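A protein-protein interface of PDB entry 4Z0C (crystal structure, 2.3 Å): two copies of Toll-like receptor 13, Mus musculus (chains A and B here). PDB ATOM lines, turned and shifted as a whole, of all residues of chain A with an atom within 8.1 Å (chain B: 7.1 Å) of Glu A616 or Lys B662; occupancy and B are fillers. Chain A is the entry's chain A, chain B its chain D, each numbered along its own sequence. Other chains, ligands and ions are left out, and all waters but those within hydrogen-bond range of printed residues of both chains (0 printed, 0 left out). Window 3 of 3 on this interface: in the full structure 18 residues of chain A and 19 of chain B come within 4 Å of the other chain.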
ATOM      1  N   ASP A 587     -22.661 -22.915  28.092  1.00  0.00           N
ATOM      2  CA  ASP A 587     -23.063 -21.501  27.983  1.00  0.00           C
ATOM      3  C   ASP A 587     -23.377 -20.839  29.310  1.00  0.00           C
ATOM      4  O   ASP A 587     -24.539 -20.631  29.677  1.00  0.00           O
ATOM      5  CB  ASP A 587     -24.147 -21.221  26.917  1.00  0.00           C
ATOM      6  CG  ASP A 587     -25.411 -21.966  27.163  1.00  0.00           C
ATOM      7  OD1 ASP A 587     -25.378 -22.897  27.987  1.00  0.00           O
ATOM      8  OD2 ASP A 587     -26.426 -21.646  26.504  1.00  0.00           O
ATOM      9  N   GLY A 588     -22.282 -20.482  29.979  1.00  0.00           N
ATOM     10  CA  GLY A 588     -22.238 -19.874  31.294  1.00  0.00           C
ATOM     11  C   GLY A 588     -23.476 -19.629  32.128  1.00  0.00           C
ATOM     12  O   GLY A 588     -23.949 -20.525  32.835  1.00  0.00           O
ATOM     13  N   ASP A 589     -23.987 -18.406  32.060  1.00  0.00           N
ATOM     14  CA  ASP A 589     -25.020 -17.971  32.982  1.00  0.00           C
ATOM     15  C   ASP A 589     -26.271 -18.838  32.876  1.00  0.00           C
ATOM     16  O   ASP A 589     -26.905 -19.149  33.884  1.00  0.00           O
ATOM     17  CB  ASP A 589     -25.346 -16.491  32.771  1.00  0.00           C
ATOM     18  CG  ASP A 589     -24.328 -15.567  33.439  1.00  0.00           C
ATOM     19  OD1 ASP A 589     -23.719 -15.994  34.441  1.00  0.00           O
ATOM     20  OD2 ASP A 589     -24.142 -14.416  32.973  1.00  0.00           O
ATOM     21  N   ARG A 590     -26.594 -19.265  31.661  1.00  0.00           N
ATOM     22  CA  ARG A 590     -27.753 -20.121  31.447  1.00  0.00           C
ATOM     23  C   ARG A 590     -27.527 -21.535  31.970  1.00  0.00           C
ATOM     24  O   ARG A 590     -28.450 -22.132  32.499  1.00  0.00           O
ATOM     25  CB  ARG A 590     -28.122 -20.180  29.966  1.00  0.00           C
ATOM     26  CG  ARG A 590     -28.658 -18.872  29.401  1.00  0.00           C
ATOM     27  CD  ARG A 590     -29.070 -19.057  27.953  1.00  0.00           C
ATOM     28  NE  ARG A 590     -28.677 -17.919  27.136  1.00  0.00           N
ATOM     29  CZ  ARG A 590     -27.714 -17.950  26.222  1.00  0.00           C
ATOM     30  NH1 ARG A 590     -27.065 -19.073  25.982  1.00  0.00           N
ATOM     31  NH2 ARG A 590     -27.415 -16.864  25.528  1.00  0.00           N
ATOM     32  N   ASN A 613     -17.084 -23.799  29.525  1.00  0.00           N
ATOM     33  CA  ASN A 613     -18.341 -23.353  30.091  1.00  0.00           C
ATOM     34  C   ASN A 613     -18.724 -22.011  29.516  1.00  0.00           C
ATOM     35  O   ASN A 613     -19.725 -21.433  29.930  1.00  0.00           O
ATOM     36  CB  ASN A 613     -18.242 -23.255  31.597  1.00  0.00           C
ATOM     37  CG  ASN A 613     -18.414 -24.580  32.263  1.00  0.00           C
ATOM     38  OD1 ASN A 613     -19.347 -25.304  31.958  1.00  0.00           O
ATOM     39  ND2 ASN A 613     -17.501 -24.922  33.161  1.00  0.00           N
ATOM     40  N   ASN A 614     -17.927 -21.515  28.568  1.00  0.00           N
ATOM     41  CA  ASN A 614     -18.166 -20.192  27.994  1.00  0.00           C
ATOM     42  C   ASN A 614     -18.376 -19.075  29.016  1.00  0.00           C
ATOM     43  O   ASN A 614     -19.171 -18.167  28.791  1.00  0.00           O
ATOM     44  CB  ASN A 614     -19.335 -20.244  27.007  1.00  0.00           C
ATOM     45  CG  ASN A 614     -18.894 -20.524  25.581  1.00  0.00           C
ATOM     46  OD1 ASN A 614     -19.379 -19.889  24.647  1.00  0.00           O
ATOM     47  ND2 ASN A 614     -17.954 -21.445  25.408  1.00  0.00           N
ATOM     48  N   LEU A 615     -17.668 -19.156  30.138  1.00  0.00           N
ATOM     49  CA  LEU A 615     -17.695 -18.117  31.172  1.00  0.00           C
ATOM     50  C   LEU A 615     -17.257 -16.765  30.606  1.00  0.00           C
ATOM     51  O   LEU A 615     -16.284 -16.690  29.858  1.00  0.00           O
ATOM     52  CB  LEU A 615     -16.750 -18.498  32.311  1.00  0.00           C
ATOM     53  CG  LEU A 615     -17.232 -19.206  33.584  1.00  0.00           C
ATOM     54  CD1 LEU A 615     -18.566 -19.905  33.419  1.00  0.00           C
ATOM     55  CD2 LEU A 615     -16.144 -20.178  34.100  1.00  0.00           C
ATOM     56  N   GLU A 616     -17.953 -15.695  30.988  1.00  0.00           N
ATOM     57  CA  GLU A 616     -17.636 -14.361  30.479  1.00  0.00           C
ATOM     58  C   GLU A 616     -16.840 -13.516  31.496  1.00  0.00           C
ATOM     59  O   GLU A 616     -16.073 -12.626  31.121  1.00  0.00           O
ATOM     60  CB  GLU A 616     -18.924 -13.652  30.034  1.00  0.00           C
ATOM     61  CG  GLU A 616     -18.828 -13.070  28.633  1.00  0.00           C
ATOM     62  CD  GLU A 616     -19.492 -13.962  27.592  1.00  0.00           C
ATOM     63  OE1 GLU A 616     -20.119 -14.956  28.004  1.00  0.00           O
ATOM     64  OE2 GLU A 616     -19.365 -13.695  26.372  1.00  0.00           O
ATOM     65  N   SER A 617     -17.007 -13.835  32.775  1.00  0.00           N
ATOM     66  CA  SER A 617     -16.356 -13.128  33.875  1.00  0.00           C
ATOM     67  C   SER A 617     -16.112 -14.118  35.001  1.00  0.00           C
ATOM     68  O   SER A 617     -16.601 -15.242  34.956  1.00  0.00           O
ATOM     69  CB  SER A 617     -17.255 -12.009  34.419  1.00  0.00           C
ATOM     70  OG  SER A 617     -17.825 -11.255  33.372  1.00  0.00           O
ATOM     71  N   LEU A 618     -15.392 -13.682  36.028  1.00  0.00           N
ATOM     72  CA  LEU A 618     -15.178 -14.497  37.219  1.00  0.00           C
ATOM     73  C   LEU A 618     -15.795 -13.830  38.459  1.00  0.00           C
ATOM     74  O   LEU A 618     -15.783 -12.610  38.585  1.00  0.00           O
ATOM     75  CB  LEU A 618     -13.681 -14.731  37.415  1.00  0.00           C
ATOM     76  CG  LEU A 618     -13.024 -16.073  37.025  1.00  0.00           C
ATOM     77  CD1 LEU A 618     -13.688 -16.772  35.823  1.00  0.00           C
ATOM     78  CD2 LEU A 618     -11.521 -15.853  36.782  1.00  0.00           C
ATOM     79  N   VAL A 619     -16.383 -14.627  39.345  1.00  0.00           N
ATOM     80  CA  VAL A 619     -16.984 -14.105  40.574  1.00  0.00           C
ATOM     81  C   VAL A 619     -15.899 -13.728  41.589  1.00  0.00           C
ATOM     82  O   VAL A 619     -15.073 -14.575  41.943  1.00  0.00           O
ATOM     83  CB  VAL A 619     -17.938 -15.152  41.210  1.00  0.00           C
ATOM     84  CG1 VAL A 619     -18.300 -14.763  42.628  1.00  0.00           C
ATOM     85  CG2 VAL A 619     -19.198 -15.355  40.352  1.00  0.00           C
ATOM     86  N   ASN A 637     -13.126 -20.824  27.653  1.00  0.00           N
ATOM     87  CA  ASN A 637     -14.210 -19.959  28.080  1.00  0.00           C
ATOM     88  C   ASN A 637     -14.135 -18.658  27.303  1.00  0.00           C
ATOM     89  O   ASN A 637     -13.423 -18.585  26.298  1.00  0.00           O
ATOM     90  CB  ASN A 637     -14.159 -19.708  29.578  1.00  0.00           C
ATOM     91  CG  ASN A 637     -14.597 -20.913  30.378  1.00  0.00           C
ATOM     92  OD1 ASN A 637     -15.797 -21.203  30.500  1.00  0.00           O
ATOM     93  ND2 ASN A 637     -13.624 -21.636  30.925  1.00  0.00           N
ATOM     94  N   ASN A 638     -14.880 -17.652  27.753  1.00  0.00           N
ATOM     95  CA  ASN A 638     -14.889 -16.338  27.113  1.00  0.00           C
ATOM     96  C   ASN A 638     -14.353 -15.240  28.012  1.00  0.00           C
ATOM     97  O   ASN A 638     -14.815 -14.104  27.945  1.00  0.00           O
ATOM     98  CB  ASN A 638     -16.291 -15.986  26.614  1.00  0.00           C
ATOM     99  CG  ASN A 638     -16.699 -16.834  25.408  1.00  0.00           C
ATOM    100  OD1 ASN A 638     -15.836 -17.377  24.708  1.00  0.00           O
ATOM    101  ND2 ASN A 638     -18.008 -16.962  25.169  1.00  0.00           N
ATOM    102  N   LEU A 639     -13.382 -15.591  28.856  1.00  0.00           N
ATOM    103  CA  LEU A 639     -12.759 -14.635  29.768  1.00  0.00           C
ATOM    104  C   LEU A 639     -11.995 -13.589  28.972  1.00  0.00           C
ATOM    105  O   LEU A 639     -11.236 -13.936  28.067  1.00  0.00           O
ATOM    106  CB  LEU A 639     -11.829 -15.358  30.730  1.00  0.00           C
ATOM    107  CG  LEU A 639     -12.309 -15.782  32.121  1.00  0.00           C
ATOM    108  CD1 LEU A 639     -13.804 -15.771  32.281  1.00  0.00           C
ATOM    109  CD2 LEU A 639     -11.765 -17.155  32.438  1.00  0.00           C
ATOM    110  N   LYS A 640     -12.213 -12.312  29.299  1.00  0.00           N
ATOM    111  CA  LYS A 640     -11.573 -11.190  28.603  1.00  0.00           C
ATOM    112  C   LYS A 640     -10.416 -10.588  29.409  1.00  0.00           C
ATOM    113  O   LYS A 640      -9.475 -10.009  28.852  1.00  0.00           O
ATOM    114  CB  LYS A 640     -12.590 -10.084  28.301  1.00  0.00           C
ATOM    115  CG  LYS A 640     -13.590 -10.400  27.195  1.00  0.00           C
ATOM    116  CD  LYS A 640     -15.022 -10.446  27.745  1.00  0.00           C
ATOM    117  CE  LYS A 640     -15.423  -9.075  28.309  1.00  0.00           C
ATOM    118  NZ  LYS A 640     -16.748  -9.053  29.021  1.00  0.00           N
ATOM    119  N   VAL A 641     -10.503 -10.718  30.725  1.00  0.00           N
ATOM    120  CA  VAL A 641      -9.551 -10.094  31.619  1.00  0.00           C
ATOM    121  C   VAL A 641      -9.225 -11.019  32.769  1.00  0.00           C
ATOM    122  O   VAL A 641     -10.124 -11.608  33.370  1.00  0.00           O
ATOM    123  CB  VAL A 641     -10.139  -8.758  32.208  1.00  0.00           C
ATOM    124  CG1 VAL A 641      -9.302  -8.249  33.387  1.00  0.00           C
ATOM    125  CG2 VAL A 641     -10.260  -7.692  31.121  1.00  0.00           C
ATOM    126  N   ASN A 661      -9.280 -18.734  25.529  1.00  0.00           N
ATOM    127  CA  ASN A 661     -10.120 -17.621  25.988  1.00  0.00           C
ATOM    128  C   ASN A 661     -10.080 -16.405  25.064  1.00  0.00           C
ATOM    129  O   ASN A 661      -9.676 -16.515  23.907  1.00  0.00           O
ATOM    130  CB  ASN A 661      -9.801 -17.255  27.434  1.00  0.00           C
ATOM    131  CG  ASN A 661     -10.442 -18.200  28.421  1.00  0.00           C
ATOM    132  OD1 ASN A 661     -11.430 -17.864  29.049  1.00  0.00           O
ATOM    133  ND2 ASN A 661      -9.922 -19.415  28.513  1.00  0.00           N
ATOM    134  N   LYS A 662     -10.496 -15.250  25.575  1.00  0.00           N
ATOM    135  CA  LYS A 662     -10.552 -14.036  24.766  1.00  0.00           C
ATOM    136  C   LYS A 662      -9.825 -12.874  25.438  1.00  0.00           C
ATOM    137  O   LYS A 662     -10.339 -11.759  25.509  1.00  0.00           O
ATOM    138  CB  LYS A 662     -12.003 -13.639  24.501  1.00  0.00           C
ATOM    139  CG  LYS A 662     -12.907 -14.771  24.010  1.00  0.00           C
ATOM    140  CD  LYS A 662     -13.672 -14.348  22.768  1.00  0.00           C
ATOM    141  CE  LYS A 662     -13.477 -15.318  21.617  1.00  0.00           C
ATOM    142  NZ  LYS A 662     -14.785 -15.880  21.193  1.00  0.00           N
ATOM    143  N   ASN B 614     -23.926 -19.778  20.555  1.00  0.00           N
ATOM    144  CA  ASN B 614     -22.860 -18.915  21.067  1.00  0.00           C
ATOM    145  C   ASN B 614     -22.042 -18.253  19.969  1.00  0.00           C
ATOM    146  O   ASN B 614     -20.837 -18.109  20.102  1.00  0.00           O
ATOM    147  CB  ASN B 614     -21.957 -19.674  22.048  1.00  0.00           C
ATOM    148  CG  ASN B 614     -22.524 -19.682  23.453  1.00  0.00           C
ATOM    149  OD1 ASN B 614     -22.849 -20.739  24.006  1.00  0.00           O
ATOM    150  ND2 ASN B 614     -22.682 -18.493  24.031  1.00  0.00           N
ATOM    151  N   LEU B 615     -22.708 -17.890  18.876  1.00  0.00           N
ATOM    152  CA  LEU B 615     -22.089 -17.169  17.768  1.00  0.00           C
ATOM    153  C   LEU B 615     -21.550 -15.803  18.171  1.00  0.00           C
ATOM    154  O   LEU B 615     -22.229 -15.022  18.837  1.00  0.00           O
ATOM    155  CB  LEU B 615     -23.112 -16.972  16.655  1.00  0.00           C
ATOM    156  CG  LEU B 615     -23.091 -17.924  15.456  1.00  0.00           C
ATOM    157  CD1 LEU B 615     -22.283 -19.215  15.704  1.00  0.00           C
ATOM    158  CD2 LEU B 615     -24.536 -18.234  15.081  1.00  0.00           C
ATOM    159  N   GLU B 616     -20.335 -15.506  17.729  1.00  0.00           N
ATOM    160  CA  GLU B 616     -19.693 -14.243  18.047  1.00  0.00           C
ATOM    161  C   GLU B 616     -19.752 -13.275  16.878  1.00  0.00           C
ATOM    162  O   GLU B 616     -19.697 -12.065  17.071  1.00  0.00           O
ATOM    163  CB  GLU B 616     -18.244 -14.469  18.489  1.00  0.00           C
ATOM    164  CG  GLU B 616     -17.847 -13.708  19.746  1.00  0.00           C
ATOM    165  CD  GLU B 616     -17.849 -14.567  21.004  1.00  0.00           C
ATOM    166  OE1 GLU B 616     -18.093 -15.789  20.900  1.00  0.00           O
ATOM    167  OE2 GLU B 616     -17.588 -14.013  22.099  1.00  0.00           O
ATOM    168  N   ASN B 637     -27.313 -16.080  21.173  1.00  0.00           N
ATOM    169  CA  ASN B 637     -25.924 -16.158  20.754  1.00  0.00           C
ATOM    170  C   ASN B 637     -25.146 -15.041  21.444  1.00  0.00           C
ATOM    171  O   ASN B 637     -25.662 -14.419  22.379  1.00  0.00           O
ATOM    172  CB  ASN B 637     -25.793 -16.076  19.228  1.00  0.00           C
ATOM    173  CG  ASN B 637     -26.203 -17.376  18.528  1.00  0.00           C
ATOM    174  OD1 ASN B 637     -25.448 -18.351  18.522  1.00  0.00           O
ATOM    175  ND2 ASN B 637     -27.390 -17.382  17.915  1.00  0.00           N
ATOM    176  N   ASN B 638     -23.916 -14.788  20.989  1.00  0.00           N
ATOM    177  CA  ASN B 638     -23.074 -13.746  21.570  1.00  0.00           C
ATOM    178  C   ASN B 638     -22.812 -12.591  20.596  1.00  0.00           C
ATOM    179  O   ASN B 638     -21.747 -11.975  20.630  1.00  0.00           O
ATOM    180  CB  ASN B 638     -21.741 -14.324  22.041  1.00  0.00           C
ATOM    181  CG  ASN B 638     -21.883 -15.218  23.255  1.00  0.00           C
ATOM    182  OD1 ASN B 638     -21.060 -16.101  23.482  1.00  0.00           O
ATOM    183  ND2 ASN B 638     -22.925 -15.001  24.033  1.00  0.00           N
ATOM    184  N   LEU B 639     -23.782 -12.310  19.729  1.00  0.00           N
ATOM    185  CA  LEU B 639     -23.654 -11.234  18.748  1.00  0.00           C
ATOM    186  C   LEU B 639     -23.585  -9.857  19.402  1.00  0.00           C
ATOM    187  O   LEU B 639     -24.405  -9.532  20.264  1.00  0.00           O
ATOM    188  CB  LEU B 639     -24.831 -11.272  17.779  1.00  0.00           C
ATOM    189  CG  LEU B 639     -24.674 -12.004  16.453  1.00  0.00           C
ATOM    190  CD1 LEU B 639     -23.491 -12.952  16.491  1.00  0.00           C
ATOM    191  CD2 LEU B 639     -25.962 -12.724  16.134  1.00  0.00           C
ATOM    192  N   LYS B 640     -22.612  -9.053  18.976  1.00  0.00           N
ATOM    193  CA  LYS B 640     -22.375  -7.720  19.544  1.00  0.00           C
ATOM    194  C   LYS B 640     -22.899  -6.618  18.629  1.00  0.00           C
ATOM    195  O   LYS B 640     -23.272  -5.532  19.075  1.00  0.00           O
ATOM    196  CB  LYS B 640     -20.879  -7.521  19.818  1.00  0.00           C
ATOM    197  CG  LYS B 640     -20.372  -8.279  21.041  1.00  0.00           C
ATOM    198  CD  LYS B 640     -19.412  -9.404  20.673  1.00  0.00           C
ATOM    199  CE  LYS B 640     -18.128  -8.893  20.025  1.00  0.00           C
ATOM    200  NZ  LYS B 640     -17.302 -10.031  19.509  1.00  0.00           N
ATOM    201  N   VAL B 641     -22.927  -6.916  17.339  1.00  0.00           N
ATOM    202  CA  VAL B 641     -23.320  -5.938  16.347  1.00  0.00           C
ATOM    203  C   VAL B 641     -24.186  -6.597  15.295  1.00  0.00           C
ATOM    204  O   VAL B 641     -23.942  -7.721  14.874  1.00  0.00           O
ATOM    205  CB  VAL B 641     -22.103  -5.316  15.653  1.00  0.00           C
ATOM    206  CG1 VAL B 641     -22.527  -4.559  14.391  1.00  0.00           C
ATOM    207  CG2 VAL B 641     -21.342  -4.406  16.626  1.00  0.00           C
ATOM    208  N   VAL B 658     -33.139 -11.499  17.767  1.00  0.00           N
ATOM    209  CA  VAL B 658     -31.771 -11.425  18.220  1.00  0.00           C
ATOM    210  C   VAL B 658     -31.760 -11.155  19.729  1.00  0.00           C
ATOM    211  O   VAL B 658     -30.802 -10.628  20.308  1.00  0.00           O
ATOM    212  CB  VAL B 658     -30.993 -10.451  17.348  1.00  0.00           C
ATOM    213  CG1 VAL B 658     -31.295  -9.042  17.731  1.00  0.00           C
ATOM    214  CG2 VAL B 658     -29.508 -10.770  17.405  1.00  0.00           C
ATOM    215  N   TYR B 659     -32.862 -11.582  20.346  1.00  0.00           N
ATOM    216  CA  TYR B 659     -33.037 -11.603  21.793  1.00  0.00           C
ATOM    217  C   TYR B 659     -31.963 -12.481  22.413  1.00  0.00           C
ATOM    218  O   TYR B 659     -31.451 -13.391  21.767  1.00  0.00           O
ATOM    219  CB  TYR B 659     -34.440 -12.145  22.127  1.00  0.00           C
ATOM    220  CG  TYR B 659     -34.713 -12.377  23.601  1.00  0.00           C
ATOM    221  CD1 TYR B 659     -34.783 -11.318  24.496  1.00  0.00           C
ATOM    222  CD2 TYR B 659     -34.914 -13.661  24.092  1.00  0.00           C
ATOM    223  CE1 TYR B 659     -35.029 -11.536  25.850  1.00  0.00           C
ATOM    224  CE2 TYR B 659     -35.168 -13.889  25.437  1.00  0.00           C
ATOM    225  CZ  TYR B 659     -35.219 -12.826  26.314  1.00  0.00           C
ATOM    226  OH  TYR B 659     -35.472 -13.063  27.653  1.00  0.00           O
ATOM    227  N   GLY B 660     -31.590 -12.185  23.650  1.00  0.00           N
ATOM    228  CA  GLY B 660     -30.585 -12.963  24.347  1.00  0.00           C
ATOM    229  C   GLY B 660     -29.167 -12.838  23.787  1.00  0.00           C
ATOM    230  O   GLY B 660     -28.312 -13.670  24.063  1.00  0.00           O
ATOM    231  N   ASN B 661     -28.894 -11.794  23.016  1.00  0.00           N
ATOM    232  CA  ASN B 661     -27.540 -11.595  22.522  1.00  0.00           C
ATOM    233  C   ASN B 661     -26.737 -10.605  23.382  1.00  0.00           C
ATOM    234  O   ASN B 661     -27.057 -10.430  24.556  1.00  0.00           O
ATOM    235  CB  ASN B 661     -27.545 -11.216  21.039  1.00  0.00           C
ATOM    236  CG  ASN B 661     -27.750 -12.429  20.139  1.00  0.00           C
ATOM    237  OD1 ASN B 661     -26.790 -12.991  19.589  1.00  0.00           O
ATOM    238  ND2 ASN B 661     -29.001 -12.840  19.986  1.00  0.00           N
ATOM    239  N   LYS B 662     -25.676 -10.013  22.820  1.00  0.00           N
ATOM    240  CA  LYS B 662     -24.818  -9.061  23.550  1.00  0.00           C
ATOM    241  C   LYS B 662     -24.673  -7.759  22.768  1.00  0.00           C
ATOM    242  O   LYS B 662     -23.554  -7.269  22.575  1.00  0.00           O
ATOM    243  CB  LYS B 662     -23.417  -9.643  23.800  1.00  0.00           C
ATOM    244  CG  LYS B 662     -23.437 -11.067  24.293  1.00  0.00           C
ATOM    245  CD  LYS B 662     -22.661 -11.249  25.567  1.00  0.00           C
ATOM    246  CE  LYS B 662     -23.558 -11.846  26.626  1.00  0.00           C
ATOM    247  NZ  LYS B 662     -23.107 -13.188  27.072  1.00  0.00           N
ATOM    248  N   LEU B 663     -25.792  -7.226  22.292  1.00  0.00           N
ATOM    249  CA  LEU B 663     -25.774  -6.042  21.435  1.00  0.00           C
ATOM    250  C   LEU B 663     -25.241  -4.793  22.143  1.00  0.00           C
ATOM    251  O   LEU B 663     -25.736  -4.416  23.207  1.00  0.00           O
ATOM    252  CB  LEU B 663     -27.169  -5.782  20.883  1.00  0.00           C
ATOM    253  CG  LEU B 663     -27.469  -6.288  19.475  1.00  0.00           C
ATOM    254  CD1 LEU B 663     -26.554  -7.424  19.093  1.00  0.00           C
ATOM    255  CD2 LEU B 663     -28.920  -6.693  19.387  1.00  0.00           C
ATOM    256  N   GLN B 664     -24.236  -4.151  21.553  1.00  0.00           N
ATOM    257  CA  GLN B 664     -23.569  -3.027  22.217  1.00  0.00           C
ATOM    258  C   GLN B 664     -24.243  -1.674  21.974  1.00  0.00           C
ATOM    259  O   GLN B 664     -24.649  -1.350  20.850  1.00  0.00           O
ATOM    260  CB  GLN B 664     -22.097  -2.959  21.805  1.00  0.00           C
ATOM    261  CG  GLN B 664     -21.491  -4.319  21.549  1.00  0.00           C
ATOM    262  CD  GLN B 664     -20.046  -4.402  21.943  1.00  0.00           C
ATOM    263  OE1 GLN B 664     -19.712  -4.415  23.125  1.00  0.00           O
ATOM    264  NE2 GLN B 664     -19.172  -4.459  20.951  1.00  0.00           N
ATOM    265  N   CYS B 665     -24.362  -0.891  23.044  1.00  0.00           N
ATOM    266  CA  CYS B 665     -24.845   0.486  22.946  1.00  0.00           C
ATOM    267  C   CYS B 665     -23.688   1.373  22.489  1.00  0.00           C
ATOM    268  O   CYS B 665     -23.049   2.042  23.291  1.00  0.00           O
ATOM    269  CB  CYS B 665     -25.403   0.962  24.288  1.00  0.00           C
ATOM    270  SG  CYS B 665     -26.882   0.061  24.866  1.00  0.00           S
ATOM    271  N   ASN B 669     -24.278   0.061  16.341  1.00  0.00           N
ATOM    272  CA  ASN B 669     -25.650  -0.404  16.321  1.00  0.00           C
ATOM    273  C   ASN B 669     -26.655   0.698  16.033  1.00  0.00           C
ATOM    274  O   ASN B 669     -27.860   0.512  16.198  1.00  0.00           O
ATOM    275  CB  ASN B 669     -25.983  -1.162  17.608  1.00  0.00           C
ATOM    276  CG  ASN B 669     -25.400  -2.560  17.605  1.00  0.00           C
ATOM    277  OD1 ASN B 669     -25.419  -3.238  16.575  1.00  0.00           O
ATOM    278  ND2 ASN B 669     -24.869  -2.997  18.744  1.00  0.00           N
ATOM    279  N   PRO B 691     -30.783  -4.757  26.866  1.00  0.00           N
ATOM    280  CA  PRO B 691     -29.963  -3.963  27.782  1.00  0.00           C
ATOM    281  C   PRO B 691     -28.567  -3.649  27.240  1.00  0.00           C
ATOM    282  O   PRO B 691     -28.044  -4.351  26.363  1.00  0.00           O
ATOM    283  CB  PRO B 691     -29.840  -4.881  28.997  1.00  0.00           C
ATOM    284  CG  PRO B 691     -29.792  -6.226  28.396  1.00  0.00           C
ATOM    285  CD  PRO B 691     -30.724  -6.189  27.198  1.00  0.00           C
ATOM    286  N   GLN B 693     -24.504  -3.412  27.526  1.00  0.00           N
ATOM    287  CA  GLN B 693     -23.561  -4.423  27.994  1.00  0.00           C
ATOM    288  C   GLN B 693     -22.731  -4.030  29.207  1.00  0.00           C
ATOM    289  O   GLN B 693     -22.088  -4.891  29.814  1.00  0.00           O
ATOM    290  CB  GLN B 693     -22.653  -4.863  26.849  1.00  0.00           C
ATOM    291  CG  GLN B 693     -22.758  -6.357  26.596  1.00  0.00           C
ATOM    292  CD  GLN B 693     -24.206  -6.846  26.601  1.00  0.00           C
ATOM    293  OE1 GLN B 693     -25.096  -6.231  25.998  1.00  0.00           O
ATOM    294  NE2 GLN B 693     -24.448  -7.942  27.312  1.00  0.00           N
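Asn B614 touches its own counterpart, Asn A614.
Glu A616 touches Lys B662, and with the chains exchanged Lys A662 touches Glu B616.
Asn B638 touches its own counterpart, Asn A638.
Positions printed for both chains: 614, 615, 616, 637, 638, 639, 640, 641, 661 and 662.
Of the 6 pairs that touch across the chains among the printed residues, 4 have their exchanged pair printed and touching as well.
Of the 19 printed residues of chain B, 5 touch a printed residue of chain A.
Along chain B the printed residues that touch a printed residue of chain A span positions 614 to 662.
Of the 18 printed residues of chain A, 6 touch a printed residue of chain B.
Along chain A the printed residues that touch a printed residue of chain B span positions 587 to 662.
Among the printed residues, 6 pairs touch across the chains.
Among the printed residues, Asp or Glu carboxylates within 4 Å of a Lys or Arg side-chain nitrogen of the other chain: Glu A616 with Lys B662 (3.6 Å) and Lys A662 with Glu B616 (3.3 Å).
CB of Asp A587 touches OD1 of Asn B614, 3.2 Å away.
Gly B660 touches Arg A590 (O to NH2, 3.6 Å).
Asn B614 touches Asn A614.
Asn A638 touches Asn B638 (ND2 to OD1, 3.6 Å).
The side-chain amide oxygen of Asn B638 lies within hydrogen-bond range of the side-chain amide nitrogen of Asn B614, 2.9 Å away.
N of Asn B614 lies within hydrogen-bond range of OD1 of Asn B637 (2.9 Å).
N of Asn A614 is in hydrogen-bond range of OD1 of Asn A637 (2.9 Å).
The backbone NH (N) of Asn A638 is in hydrogen-bond range of the backbone carbonyl oxygen (O) of Leu A615, 2.7 Å away.
The backbone NH (N) of Lys B662 sits at hydrogen-bond distance from the backbone carbonyl oxygen (O) of Leu B639, at 2.9 Å.
The side-chain amide nitrogen of Asn A638 sits at hydrogen-bond distance from the side-chain amide oxygen of Asn A614 (3.3 Å).
The side-chain carboxylate (OE1) of Glu B616 is in salt-bridge range of the side-chain amino group (NZ) of Lys A662 (3.3 Å).
NZ of Lys B662 lies within salt-bridge range of OE1 of Glu A616, 3.6 Å away.
Printed residues of chain B within 4 Å of Arg A590: Gly B660 (3.6 Å).
Of the printed residues of chain A, Glu B616 touches Lys A662 (3.3 Å).
Printed residues of chain A within 4 Å of Asn B638: Asn A638 (3.6 Å).
Lys B662 touches just one residue of chain A: Glu A616 (3.6 Å).
The nearest residue of chain B that does not touch Glu A616 is Asn B638 (4.1 Å).
The nearest residue of chain A that does not touch Lys B662 is Arg A590 (5.9 Å).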
